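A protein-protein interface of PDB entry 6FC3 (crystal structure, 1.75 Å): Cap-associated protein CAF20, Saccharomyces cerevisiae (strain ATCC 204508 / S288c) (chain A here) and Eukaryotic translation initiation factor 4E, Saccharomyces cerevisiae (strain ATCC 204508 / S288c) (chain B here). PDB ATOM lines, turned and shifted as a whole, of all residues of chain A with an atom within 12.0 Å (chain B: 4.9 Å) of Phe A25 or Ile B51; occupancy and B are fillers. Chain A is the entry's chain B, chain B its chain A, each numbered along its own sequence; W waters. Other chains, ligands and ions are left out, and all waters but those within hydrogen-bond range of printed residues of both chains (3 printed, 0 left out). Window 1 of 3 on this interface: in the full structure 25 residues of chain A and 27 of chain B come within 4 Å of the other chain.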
ATOM      1  N   LYS A  16      27.481  -8.866 -26.551  1.00  0.00           N
ATOM      2  CA  LYS A  16      26.528  -9.377 -25.559  1.00  0.00           C
ATOM      3  C   LYS A  16      25.716 -10.537 -26.130  1.00  0.00           C
ATOM      4  O   LYS A  16      25.071 -10.376 -27.169  1.00  0.00           O
ATOM      5  CB  LYS A  16      25.564  -8.277 -25.126  1.00  0.00           C
ATOM      6  CG  LYS A  16      24.468  -8.707 -24.142  1.00  0.00           C
ATOM      7  CD  LYS A  16      23.561  -7.523 -23.826  1.00  0.00           C
ATOM      8  CE  LYS A  16      22.628  -7.818 -22.673  1.00  0.00           C
ATOM      9  NZ  LYS A  16      21.865  -9.072 -22.895  1.00  0.00           N
ATOM     10  N   THR A  20      20.946 -19.208 -21.025  1.00  0.00           N
ATOM     11  CA  THR A  20      21.726 -19.610 -19.858  1.00  0.00           C
ATOM     12  C   THR A  20      23.232 -19.376 -20.061  1.00  0.00           C
ATOM     13  O   THR A  20      23.848 -19.924 -20.974  1.00  0.00           O
ATOM     14  CB  THR A  20      21.483 -21.093 -19.511  1.00  0.00           C
ATOM     15  OG1 THR A  20      21.761 -21.913 -20.652  1.00  0.00           O
ATOM     16  CG2 THR A  20      20.043 -21.298 -19.084  1.00  0.00           C
ATOM     17  N   LEU A  21      23.806 -18.537 -19.202  1.00  0.00           N
ATOM     18  CA  LEU A  21      25.222 -18.194 -19.228  1.00  0.00           C
ATOM     19  C   LEU A  21      25.840 -18.574 -17.892  1.00  0.00           C
ATOM     20  O   LEU A  21      25.343 -18.156 -16.840  1.00  0.00           O
ATOM     21  CB  LEU A  21      25.414 -16.702 -19.501  1.00  0.00           C
ATOM     22  CG  LEU A  21      25.001 -16.211 -20.896  1.00  0.00           C
ATOM     23  CD1 LEU A  21      25.594 -17.088 -21.982  1.00  0.00           C
ATOM     24  CD2 LEU A  21      23.490 -16.107 -21.082  1.00  0.00           C
ATOM     25  N   GLU A  22      26.911 -19.371 -17.937  1.00  0.00           N
ATOM     26  CA  GLU A  22      27.508 -19.922 -16.726  1.00  0.00           C
ATOM     27  C   GLU A  22      28.359 -18.872 -16.038  1.00  0.00           C
ATOM     28  O   GLU A  22      29.062 -18.100 -16.695  1.00  0.00           O
ATOM     29  CB  GLU A  22      28.373 -21.137 -17.046  1.00  0.00           C
ATOM     30  CG  GLU A  22      27.639 -22.311 -17.698  1.00  0.00           C
ATOM     31  CD  GLU A  22      27.222 -23.391 -16.709  1.00  0.00           C
ATOM     32  OE1 GLU A  22      27.186 -23.122 -15.487  1.00  0.00           O
ATOM     33  OE2 GLU A  22      26.929 -24.523 -17.161  1.00  0.00           O
ATOM     34  N   VAL A  23      28.286 -18.834 -14.709  1.00  0.00           N
ATOM     35  CA  VAL A  23      29.112 -17.945 -13.901  1.00  0.00           C
ATOM     36  C   VAL A  23      29.863 -18.784 -12.879  1.00  0.00           C
ATOM     37  O   VAL A  23      29.587 -19.969 -12.696  1.00  0.00           O
ATOM     38  CB  VAL A  23      28.304 -16.844 -13.188  1.00  0.00           C
ATOM     39  CG1 VAL A  23      27.861 -15.813 -14.176  1.00  0.00           C
ATOM     40  CG2 VAL A  23      27.119 -17.440 -12.418  1.00  0.00           C
ATOM     41  N   ASN A  24      30.806 -18.142 -12.189  1.00  0.00           N
ATOM     42  CA  ASN A  24      31.689 -18.842 -11.268  1.00  0.00           C
ATOM     43  C   ASN A  24      31.299 -18.645  -9.817  1.00  0.00           C
ATOM     44  O   ASN A  24      32.029 -19.086  -8.932  1.00  0.00           O
ATOM     45  CB  ASN A  24      33.131 -18.390 -11.480  1.00  0.00           C
ATOM     46  CG  ASN A  24      33.615 -18.655 -12.887  1.00  0.00           C
ATOM     47  OD1 ASN A  24      34.143 -17.768 -13.560  1.00  0.00           O
ATOM     48  ND2 ASN A  24      33.425 -19.883 -13.348  1.00  0.00           N
ATOM     49  N   PHE A  25      30.182 -17.988  -9.553  1.00  0.00           N
ATOM     50  CA  PHE A  25      29.665 -17.826  -8.209  1.00  0.00           C
ATOM     51  C   PHE A  25      28.270 -18.422  -8.153  1.00  0.00           C
ATOM     52  O   PHE A  25      27.674 -18.785  -9.175  1.00  0.00           O
ATOM     53  CB  PHE A  25      29.638 -16.355  -7.788  1.00  0.00           C
ATOM     54  CG  PHE A  25      28.687 -15.508  -8.583  1.00  0.00           C
ATOM     55  CD1 PHE A  25      29.023 -15.087  -9.854  1.00  0.00           C
ATOM     56  CD2 PHE A  25      27.459 -15.119  -8.057  1.00  0.00           C
ATOM     57  CE1 PHE A  25      28.169 -14.302 -10.592  1.00  0.00           C
ATOM     58  CE2 PHE A  25      26.587 -14.316  -8.805  1.00  0.00           C
ATOM     59  CZ  PHE A  25      26.939 -13.925 -10.071  1.00  0.00           C
ATOM     60  N   ASP A  26      27.772 -18.562  -6.930  1.00  0.00           N
ATOM     61  CA  ASP A  26      26.457 -19.150  -6.698  1.00  0.00           C
ATOM     62  C   ASP A  26      25.429 -18.034  -6.877  1.00  0.00           C
ATOM     63  O   ASP A  26      25.092 -17.305  -5.945  1.00  0.00           O
ATOM     64  CB  ASP A  26      26.397 -19.775  -5.311  1.00  0.00           C
ATOM     65  CG  ASP A  26      25.111 -20.536  -5.069  1.00  0.00           C
ATOM     66  OD1 ASP A  26      24.121 -20.310  -5.792  1.00  0.00           O
ATOM     67  OD2 ASP A  26      25.088 -21.362  -4.145  1.00  0.00           O
ATOM     68  N   ALA A  27      24.934 -17.892  -8.112  1.00  0.00           N
ATOM     69  CA  ALA A  27      24.000 -16.819  -8.436  1.00  0.00           C
ATOM     70  C   ALA A  27      22.656 -17.015  -7.750  1.00  0.00           C
ATOM     71  O   ALA A  27      21.966 -16.036  -7.459  1.00  0.00           O
ATOM     72  CB  ALA A  27      23.803 -16.737  -9.948  1.00  0.00           C
ATOM     73  N   VAL A  28      22.265 -18.267  -7.499  1.00  0.00           N
ATOM     74  CA  VAL A  28      20.995 -18.523  -6.823  1.00  0.00           C
ATOM     75  C   VAL A  28      21.061 -18.040  -5.384  1.00  0.00           C
ATOM     76  O   VAL A  28      20.158 -17.354  -4.899  1.00  0.00           O
ATOM     77  CB  VAL A  28      20.631 -20.019  -6.909  1.00  0.00           C
ATOM     78  CG1 VAL A  28      19.375 -20.320  -6.104  1.00  0.00           C
ATOM     79  CG2 VAL A  28      20.420 -20.438  -8.342  1.00  0.00           C
ATOM     80  N   GLU A  29      22.149 -18.358  -4.685  1.00  0.00           N
ATOM     81  CA  GLU A  29      22.284 -17.880  -3.317  1.00  0.00           C
ATOM     82  C   GLU A  29      22.403 -16.367  -3.261  1.00  0.00           C
ATOM     83  O   GLU A  29      21.802 -15.732  -2.399  1.00  0.00           O
ATOM     84  CB  GLU A  29      23.497 -18.503  -2.657  1.00  0.00           C
ATOM     85  CG  GLU A  29      23.638 -18.100  -1.202  1.00  0.00           C
ATOM     86  CD  GLU A  29      22.438 -18.515  -0.338  1.00  0.00           C
ATOM     87  OE1 GLU A  29      21.567 -19.289  -0.812  1.00  0.00           O
ATOM     88  OE2 GLU A  29      22.380 -18.072   0.829  1.00  0.00           O
ATOM     89  N   PHE A  30      23.193 -15.767  -4.158  1.00  0.00           N
ATOM     90  CA  PHE A  30      23.315 -14.314  -4.179  1.00  0.00           C
ATOM     91  C   PHE A  30      21.948 -13.635  -4.289  1.00  0.00           C
ATOM     92  O   PHE A  30      21.647 -12.687  -3.553  1.00  0.00           O
ATOM     93  CB  PHE A  30      24.243 -13.896  -5.324  1.00  0.00           C
ATOM     94  CG  PHE A  30      24.612 -12.475  -5.308  1.00  0.00           C
ATOM     95  CD1 PHE A  30      25.388 -11.950  -4.291  1.00  0.00           C
ATOM     96  CD2 PHE A  30      24.223 -11.654  -6.337  1.00  0.00           C
ATOM     97  CE1 PHE A  30      25.728 -10.610  -4.293  1.00  0.00           C
ATOM     98  CE2 PHE A  30      24.575 -10.315  -6.354  1.00  0.00           C
ATOM     99  CZ  PHE A  30      25.331  -9.797  -5.313  1.00  0.00           C
ATOM    100  N   ARG A  31      21.102 -14.110  -5.194  1.00  0.00           N
ATOM    101  CA  ARG A  31      19.759 -13.538  -5.316  1.00  0.00           C
ATOM    102  C   ARG A  31      18.946 -13.773  -4.048  1.00  0.00           C
ATOM    103  O   ARG A  31      18.223 -12.884  -3.582  1.00  0.00           O
ATOM    104  CB  ARG A  31      19.054 -14.144  -6.539  1.00  0.00           C
ATOM    105  CG  ARG A  31      17.536 -14.077  -6.544  1.00  0.00           C
ATOM    106  CD  ARG A  31      17.015 -12.689  -6.777  1.00  0.00           C
ATOM    107  NE  ARG A  31      17.340 -12.254  -8.131  1.00  0.00           N
ATOM    108  CZ  ARG A  31      16.865 -11.157  -8.702  1.00  0.00           C
ATOM    109  NH1 ARG A  31      16.026 -10.363  -8.045  1.00  0.00           N
ATOM    110  NH2 ARG A  31      17.244 -10.850  -9.930  1.00  0.00           N
ATOM    111  N   ALA A  32      19.049 -14.972  -3.479  1.00  0.00           N
ATOM    112  CA  ALA A  32      18.252 -15.300  -2.299  1.00  0.00           C
ATOM    113  C   ALA A  32      18.597 -14.375  -1.131  1.00  0.00           C
ATOM    114  O   ALA A  32      17.707 -13.928  -0.400  1.00  0.00           O
ATOM    115  CB  ALA A  32      18.464 -16.775  -1.931  1.00  0.00           C
ATOM    116  N   ILE A  33      19.879 -14.036  -0.968  1.00  0.00           N
ATOM    117  CA  ILE A  33      20.281 -13.131   0.110  1.00  0.00           C
ATOM    118  C   ILE A  33      19.627 -11.767  -0.071  1.00  0.00           C
ATOM    119  O   ILE A  33      19.139 -11.152   0.890  1.00  0.00           O
ATOM    120  CB  ILE A  33      21.816 -13.009   0.161  1.00  0.00           C
ATOM    121  CG1 ILE A  33      22.430 -14.320   0.662  1.00  0.00           C
ATOM    122  CG2 ILE A  33      22.228 -11.811   1.059  1.00  0.00           C
ATOM    123  CD1 ILE A  33      23.900 -14.439   0.408  1.00  0.00           C
ATOM    124  N   ILE A  34      19.653 -11.261  -1.302  1.00  0.00           N
ATOM    125  CA  ILE A  34      19.099  -9.944  -1.607  1.00  0.00           C
ATOM    126  C   ILE A  34      17.583  -9.946  -1.421  1.00  0.00           C
ATOM    127  O   ILE A  34      17.019  -9.009  -0.846  1.00  0.00           O
ATOM    128  CB  ILE A  34      19.535  -9.527  -3.029  1.00  0.00           C
ATOM    129  CG1 ILE A  34      21.002  -9.099  -2.986  1.00  0.00           C
ATOM    130  CG2 ILE A  34      18.703  -8.422  -3.575  1.00  0.00           C
ATOM    131  CD1 ILE A  34      21.670  -9.049  -4.358  1.00  0.00           C
ATOM    132  N   GLU A  35      16.909 -11.020  -1.845  1.00  0.00           N
ATOM    133  CA  GLU A  35      15.466 -11.096  -1.669  1.00  0.00           C
ATOM    134  C   GLU A  35      15.086 -11.186  -0.192  1.00  0.00           C
ATOM    135  O   GLU A  35      14.063 -10.624   0.233  1.00  0.00           O
ATOM    136  CB  GLU A  35      14.905 -12.295  -2.437  1.00  0.00           C
ATOM    137  CG  GLU A  35      15.036 -12.180  -3.962  1.00  0.00           C
ATOM    138  CD  GLU A  35      14.271 -11.020  -4.573  1.00  0.00           C
ATOM    139  OE1 GLU A  35      13.028 -10.942  -4.407  1.00  0.00           O
ATOM    140  OE2 GLU A  35      14.915 -10.181  -5.247  1.00  0.00           O
ATOM    141  N   LYS A  38      15.181  -7.753   1.255  1.00  0.00           N
ATOM    142  CA  LYS A  38      14.019  -6.951   0.878  1.00  0.00           C
ATOM    143  C   LYS A  38      12.786  -7.370   1.657  1.00  0.00           C
ATOM    144  O   LYS A  38      11.951  -6.532   2.020  1.00  0.00           O
ATOM    145  CB  LYS A  38      13.759  -7.061  -0.619  1.00  0.00           C
ATOM    146  CG  LYS A  38      14.708  -6.208  -1.435  1.00  0.00           C
ATOM    147  CD  LYS A  38      14.275  -6.139  -2.888  1.00  0.00           C
ATOM    148  CE  LYS A  38      14.676  -7.386  -3.607  1.00  0.00           C
ATOM    149  NZ  LYS A  38      14.283  -7.378  -5.048  1.00  0.00           N
ATOM    150  N   LEU B  15      33.655  -7.733  -8.980  1.00  0.00           N
ATOM    151  CA  LEU B  15      32.386  -7.231  -8.488  1.00  0.00           C
ATOM    152  C   LEU B  15      32.275  -7.516  -6.995  1.00  0.00           C
ATOM    153  O   LEU B  15      32.448  -8.662  -6.567  1.00  0.00           O
ATOM    154  CB  LEU B  15      31.218  -7.898  -9.201  1.00  0.00           C
ATOM    155  CG  LEU B  15      29.821  -7.634  -8.629  1.00  0.00           C
ATOM    156  CD1 LEU B  15      29.393  -6.186  -8.909  1.00  0.00           C
ATOM    157  CD2 LEU B  15      28.839  -8.596  -9.251  1.00  0.00           C
ATOM    158  N   VAL B  35      32.074 -10.746  -4.897  1.00  0.00           N
ATOM    159  CA  VAL B  35      31.150 -11.694  -5.517  1.00  0.00           C
ATOM    160  C   VAL B  35      31.873 -12.585  -6.505  1.00  0.00           C
ATOM    161  O   VAL B  35      31.841 -13.804  -6.387  1.00  0.00           O
ATOM    162  CB  VAL B  35      29.967 -10.961  -6.187  1.00  0.00           C
ATOM    163  CG1 VAL B  35      28.968 -11.965  -6.738  1.00  0.00           C
ATOM    164  CG2 VAL B  35      29.314 -10.007  -5.195  1.00  0.00           C
ATOM    165  N   THR B  36      32.563 -11.986  -7.467  1.00  0.00           N
ATOM    166  CA  THR B  36      33.239 -12.740  -8.513  1.00  0.00           C
ATOM    167  C   THR B  36      34.180 -11.789  -9.227  1.00  0.00           C
ATOM    168  O   THR B  36      34.072 -10.570  -9.090  1.00  0.00           O
ATOM    169  CB  THR B  36      32.218 -13.348  -9.488  1.00  0.00           C
ATOM    170  OG1 THR B  36      32.872 -14.159 -10.456  1.00  0.00           O
ATOM    171  CG2 THR B  36      31.407 -12.286 -10.192  1.00  0.00           C
ATOM    172  N   ILE B  47      28.089 -12.387 -15.945  1.00  0.00           N
ATOM    173  CA  ILE B  47      27.794 -11.865 -14.614  1.00  0.00           C
ATOM    174  C   ILE B  47      26.557 -10.972 -14.636  1.00  0.00           C
ATOM    175  O   ILE B  47      25.645 -11.131 -13.819  1.00  0.00           O
ATOM    176  CB  ILE B  47      29.018 -11.118 -14.059  1.00  0.00           C
ATOM    177  CG1 ILE B  47      30.139 -12.135 -13.777  1.00  0.00           C
ATOM    178  CG2 ILE B  47      28.643 -10.350 -12.787  1.00  0.00           C
ATOM    179  CD1 ILE B  47      31.527 -11.508 -13.638  1.00  0.00           C
ATOM    180  N   ILE B  48      26.516 -10.011 -15.557  1.00  0.00           N
ATOM    181  CA  ILE B  48      25.375  -9.111 -15.671  1.00  0.00           C
ATOM    182  C   ILE B  48      24.075  -9.893 -15.806  1.00  0.00           C
ATOM    183  O   ILE B  48      23.047  -9.529 -15.222  1.00  0.00           O
ATOM    184  CB  ILE B  48      25.572  -8.183 -16.874  1.00  0.00           C
ATOM    185  CG1 ILE B  48      26.777  -7.275 -16.663  1.00  0.00           C
ATOM    186  CG2 ILE B  48      24.293  -7.395 -17.148  1.00  0.00           C
ATOM    187  CD1 ILE B  48      26.654  -6.328 -15.464  1.00  0.00           C
ATOM    188  N   GLN B  49      24.087 -10.945 -16.620  1.00  0.00           N
ATOM    189  CA  GLN B  49      22.895 -11.769 -16.817  1.00  0.00           C
ATOM    190  C   GLN B  49      22.455 -12.500 -15.551  1.00  0.00           C
ATOM    191  O   GLN B  49      21.300 -12.958 -15.484  1.00  0.00           O
ATOM    192  CB  GLN B  49      23.186 -12.783 -17.935  1.00  0.00           C
ATOM    193  CG  GLN B  49      22.087 -13.809 -18.234  1.00  0.00           C
ATOM    194  CD  GLN B  49      20.989 -13.264 -19.126  1.00  0.00           C
ATOM    195  OE1 GLN B  49      21.002 -12.095 -19.506  1.00  0.00           O
ATOM    196  NE2 GLN B  49      20.030 -14.118 -19.469  1.00  0.00           N
ATOM    197  N   ASN B  50      23.333 -12.631 -14.556  1.00  0.00           N
ATOM    198  CA  ASN B  50      23.085 -13.503 -13.414  1.00  0.00           C
ATOM    199  C   ASN B  50      23.081 -12.771 -12.068  1.00  0.00           C
ATOM    200  O   ASN B  50      23.183 -13.425 -11.025  1.00  0.00           O
ATOM    201  CB  ASN B  50      24.120 -14.633 -13.403  1.00  0.00           C
ATOM    202  CG  ASN B  50      23.789 -15.730 -14.386  1.00  0.00           C
ATOM    203  OD1 ASN B  50      22.944 -16.567 -14.123  1.00  0.00           O
ATOM    204  ND2 ASN B  50      24.435 -15.719 -15.528  1.00  0.00           N
ATOM    205  N   ILE B  51      22.975 -11.438 -12.052  1.00  0.00           N
ATOM    206  CA  ILE B  51      22.880 -10.681 -10.798  1.00  0.00           C
ATOM    207  C   ILE B  51      21.678  -9.742 -10.883  1.00  0.00           C
ATOM    208  O   ILE B  51      21.268  -9.341 -11.993  1.00  0.00           O
ATOM    209  CB  ILE B  51      24.157  -9.877 -10.477  1.00  0.00           C
ATOM    210  CG1 ILE B  51      24.394  -8.820 -11.550  1.00  0.00           C
ATOM    211  CG2 ILE B  51      25.326 -10.793 -10.312  1.00  0.00           C
ATOM    212  CD1 ILE B  51      25.605  -7.947 -11.293  1.00  0.00           C
ATOM    213  N   PRO B  52      21.079  -9.384  -9.759  1.00  0.00           N
ATOM    214  CA  PRO B  52      19.930  -8.479  -9.819  1.00  0.00           C
ATOM    215  C   PRO B  52      20.340  -7.136 -10.413  1.00  0.00           C
ATOM    216  O   PRO B  52      21.475  -6.679 -10.241  1.00  0.00           O
ATOM    217  CB  PRO B  52      19.502  -8.358  -8.359  1.00  0.00           C
ATOM    218  CG  PRO B  52      20.032  -9.614  -7.697  1.00  0.00           C
ATOM    219  CD  PRO B  52      21.351  -9.821  -8.369  1.00  0.00           C
ATOM    220  N   GLU B  53      19.413  -6.557 -11.191  1.00  0.00           N
ATOM    221  CA  GLU B  53      19.552  -5.211 -11.728  1.00  0.00           C
ATOM    222  C   GLU B  53      19.549  -4.171 -10.612  1.00  0.00           C
ATOM    223  O   GLU B  53      18.936  -4.367  -9.562  1.00  0.00           O
ATOM    224  CB  GLU B  53      18.411  -4.920 -12.705  1.00  0.00           C
ATOM    225  CG  GLU B  53      18.505  -5.771 -13.952  1.00  0.00           C
ATOM    226  CD  GLU B  53      17.470  -5.449 -15.004  1.00  0.00           C
ATOM    227  OE1 GLU B  53      16.257  -5.414 -14.701  1.00  0.00           O
ATOM    228  OE2 GLU B  53      17.873  -5.204 -16.155  1.00  0.00           O
ATOM    229  N   TYR B  63      26.851  -1.906  -5.245  1.00  0.00           N
ATOM    230  CA  TYR B  63      27.720  -2.697  -6.104  1.00  0.00           C
ATOM    231  C   TYR B  63      29.020  -1.919  -6.291  1.00  0.00           C
ATOM    232  O   TYR B  63      28.999  -0.703  -6.514  1.00  0.00           O
ATOM    233  CB  TYR B  63      27.114  -2.945  -7.491  1.00  0.00           C
ATOM    234  CG  TYR B  63      26.048  -4.026  -7.644  1.00  0.00           C
ATOM    235  CD1 TYR B  63      26.031  -5.156  -6.835  1.00  0.00           C
ATOM    236  CD2 TYR B  63      25.093  -3.947  -8.671  1.00  0.00           C
ATOM    237  CE1 TYR B  63      25.067  -6.131  -7.004  1.00  0.00           C
ATOM    238  CE2 TYR B  63      24.144  -4.938  -8.844  1.00  0.00           C
ATOM    239  CZ  TYR B  63      24.149  -6.019  -8.021  1.00  0.00           C
ATOM    240  OH  TYR B  63      23.222  -7.010  -8.190  1.00  0.00           O
HETATM  241  O   HOH W   1      31.459 -15.384 -12.624  1.00  0.00           O
HETATM  242  O   HOH W   2      22.121 -13.468  -8.634  1.00  0.00           O
HETATM  243  O   HOH W   3      23.040 -11.816 -22.103  1.00  0.00           O
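The side-chain amide nitrogen (ND2) of Asn B50 is in hydrogen-bond range of the backbone carbonyl oxygen (O) of Leu A21.
Of the printed residues of chain B, Leu A21 touches Gln B49 and Asn B50. Of the printed residues of chain B, Val A23 touches Ile B47 and Asn B50. Phe A25 touches just these residues of chain B: Val B35 (3.7 Å), Thr B36 (3.7 Å), Asn B50 (3.9 Å) and Ile B51 (3.5 Å). Of the printed residues of chain B, Ile A34 touches Pro B52 (3.8 Å). Of chain A, only Phe A25 and Phe A30 come within 4 Å of Val B35. Thr B36 touches one residue of chain A. Ile B47 touches just one residue of chain A: Val A23. No residue of chain A comes within 4 Å of Ile B48. Printed residues of chain A within 4 Å of Gln B49: Leu A21. Of chain A, only Phe A25 (3.5 Å) comes within 4 Å of Ile B51. Of chain A, only Phe A30 (3.8 Å), Arg A31 (3.6 Å) and Ile A34 (3.8 Å) come within 4 Å of Pro B52. No residue of chain A comes within 4 Å of Glu B53.
Printed residues of chain A that touch a printed residue of chain B: Leu A21, Val A23, Phe A25, Ala A27, Phe A30, Arg A31 and Ile A34. Printed residues of chain B that touch a printed residue of chain A: Val B35, Thr B36, Ile B47, Gln B49, Asn B50, Ile B51 and Pro B52. Hydrophobic or aromatic side chains of chain B within 4 Å of the printed part of chain A: Val B35, Ile B51 and Pro B52. Among the printed residues, no Asp or Glu carboxylate lies within 4 Å of a Lys or Arg side-chain nitrogen of the other chain.
Water W2 lies within hydrogen-bond range of the backbone carbonyl oxygen (O) of Asn B50 (2.6 Å) and the backbone carbonyl oxygen (O) of Ala A27 (2.8 Å). Water W1 lies within hydrogen-bond range of the side-chain hydroxyl of Thr B36 (2.9 Å) and the backbone NH of Asn A24 (2.9 Å). Water W3 bridges NZ of Lys A16 (3.1 Å) and OE1 of Gln B49 (3.3 Å).
Among the printed residues, pairs that only touch across the chains: Leu A21 with Gln B49 (3.9 Å), Val A23 with Ile B47 (3.9 Å), Val A23 with Asn B50 (3.7 Å), Phe A25 with Val B35 (3.7 Å), Phe A25 with Thr B36 (3.7 Å), Phe A25 with Asn B50 (3.9 Å), Phe A25 with Ile B51 (3.5 Å), Ala A27 with Asn B50 (3.5 Å), Phe A30 with Val B35 (3.7 Å), Phe A30 with Pro B52 (3.8 Å), Arg A31 with Pro B52 (3.6 Å) and Ile A34 with Pro B52 (3.8 Å).
O of Pro B52 lies within hydrogen-bond range of OH of Tyr B63 (2.7 Å). The backbone carbonyl oxygen of Thr B36 is in hydrogen-bond range of the backbone NH of Leu B15 (2.9 Å). The guanidinium group of Arg A31 is in salt-bridge range of the side-chain carboxylate of Glu A35 (3.0 Å). O of Leu B15 is in hydrogen-bond range of N of Val B35.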
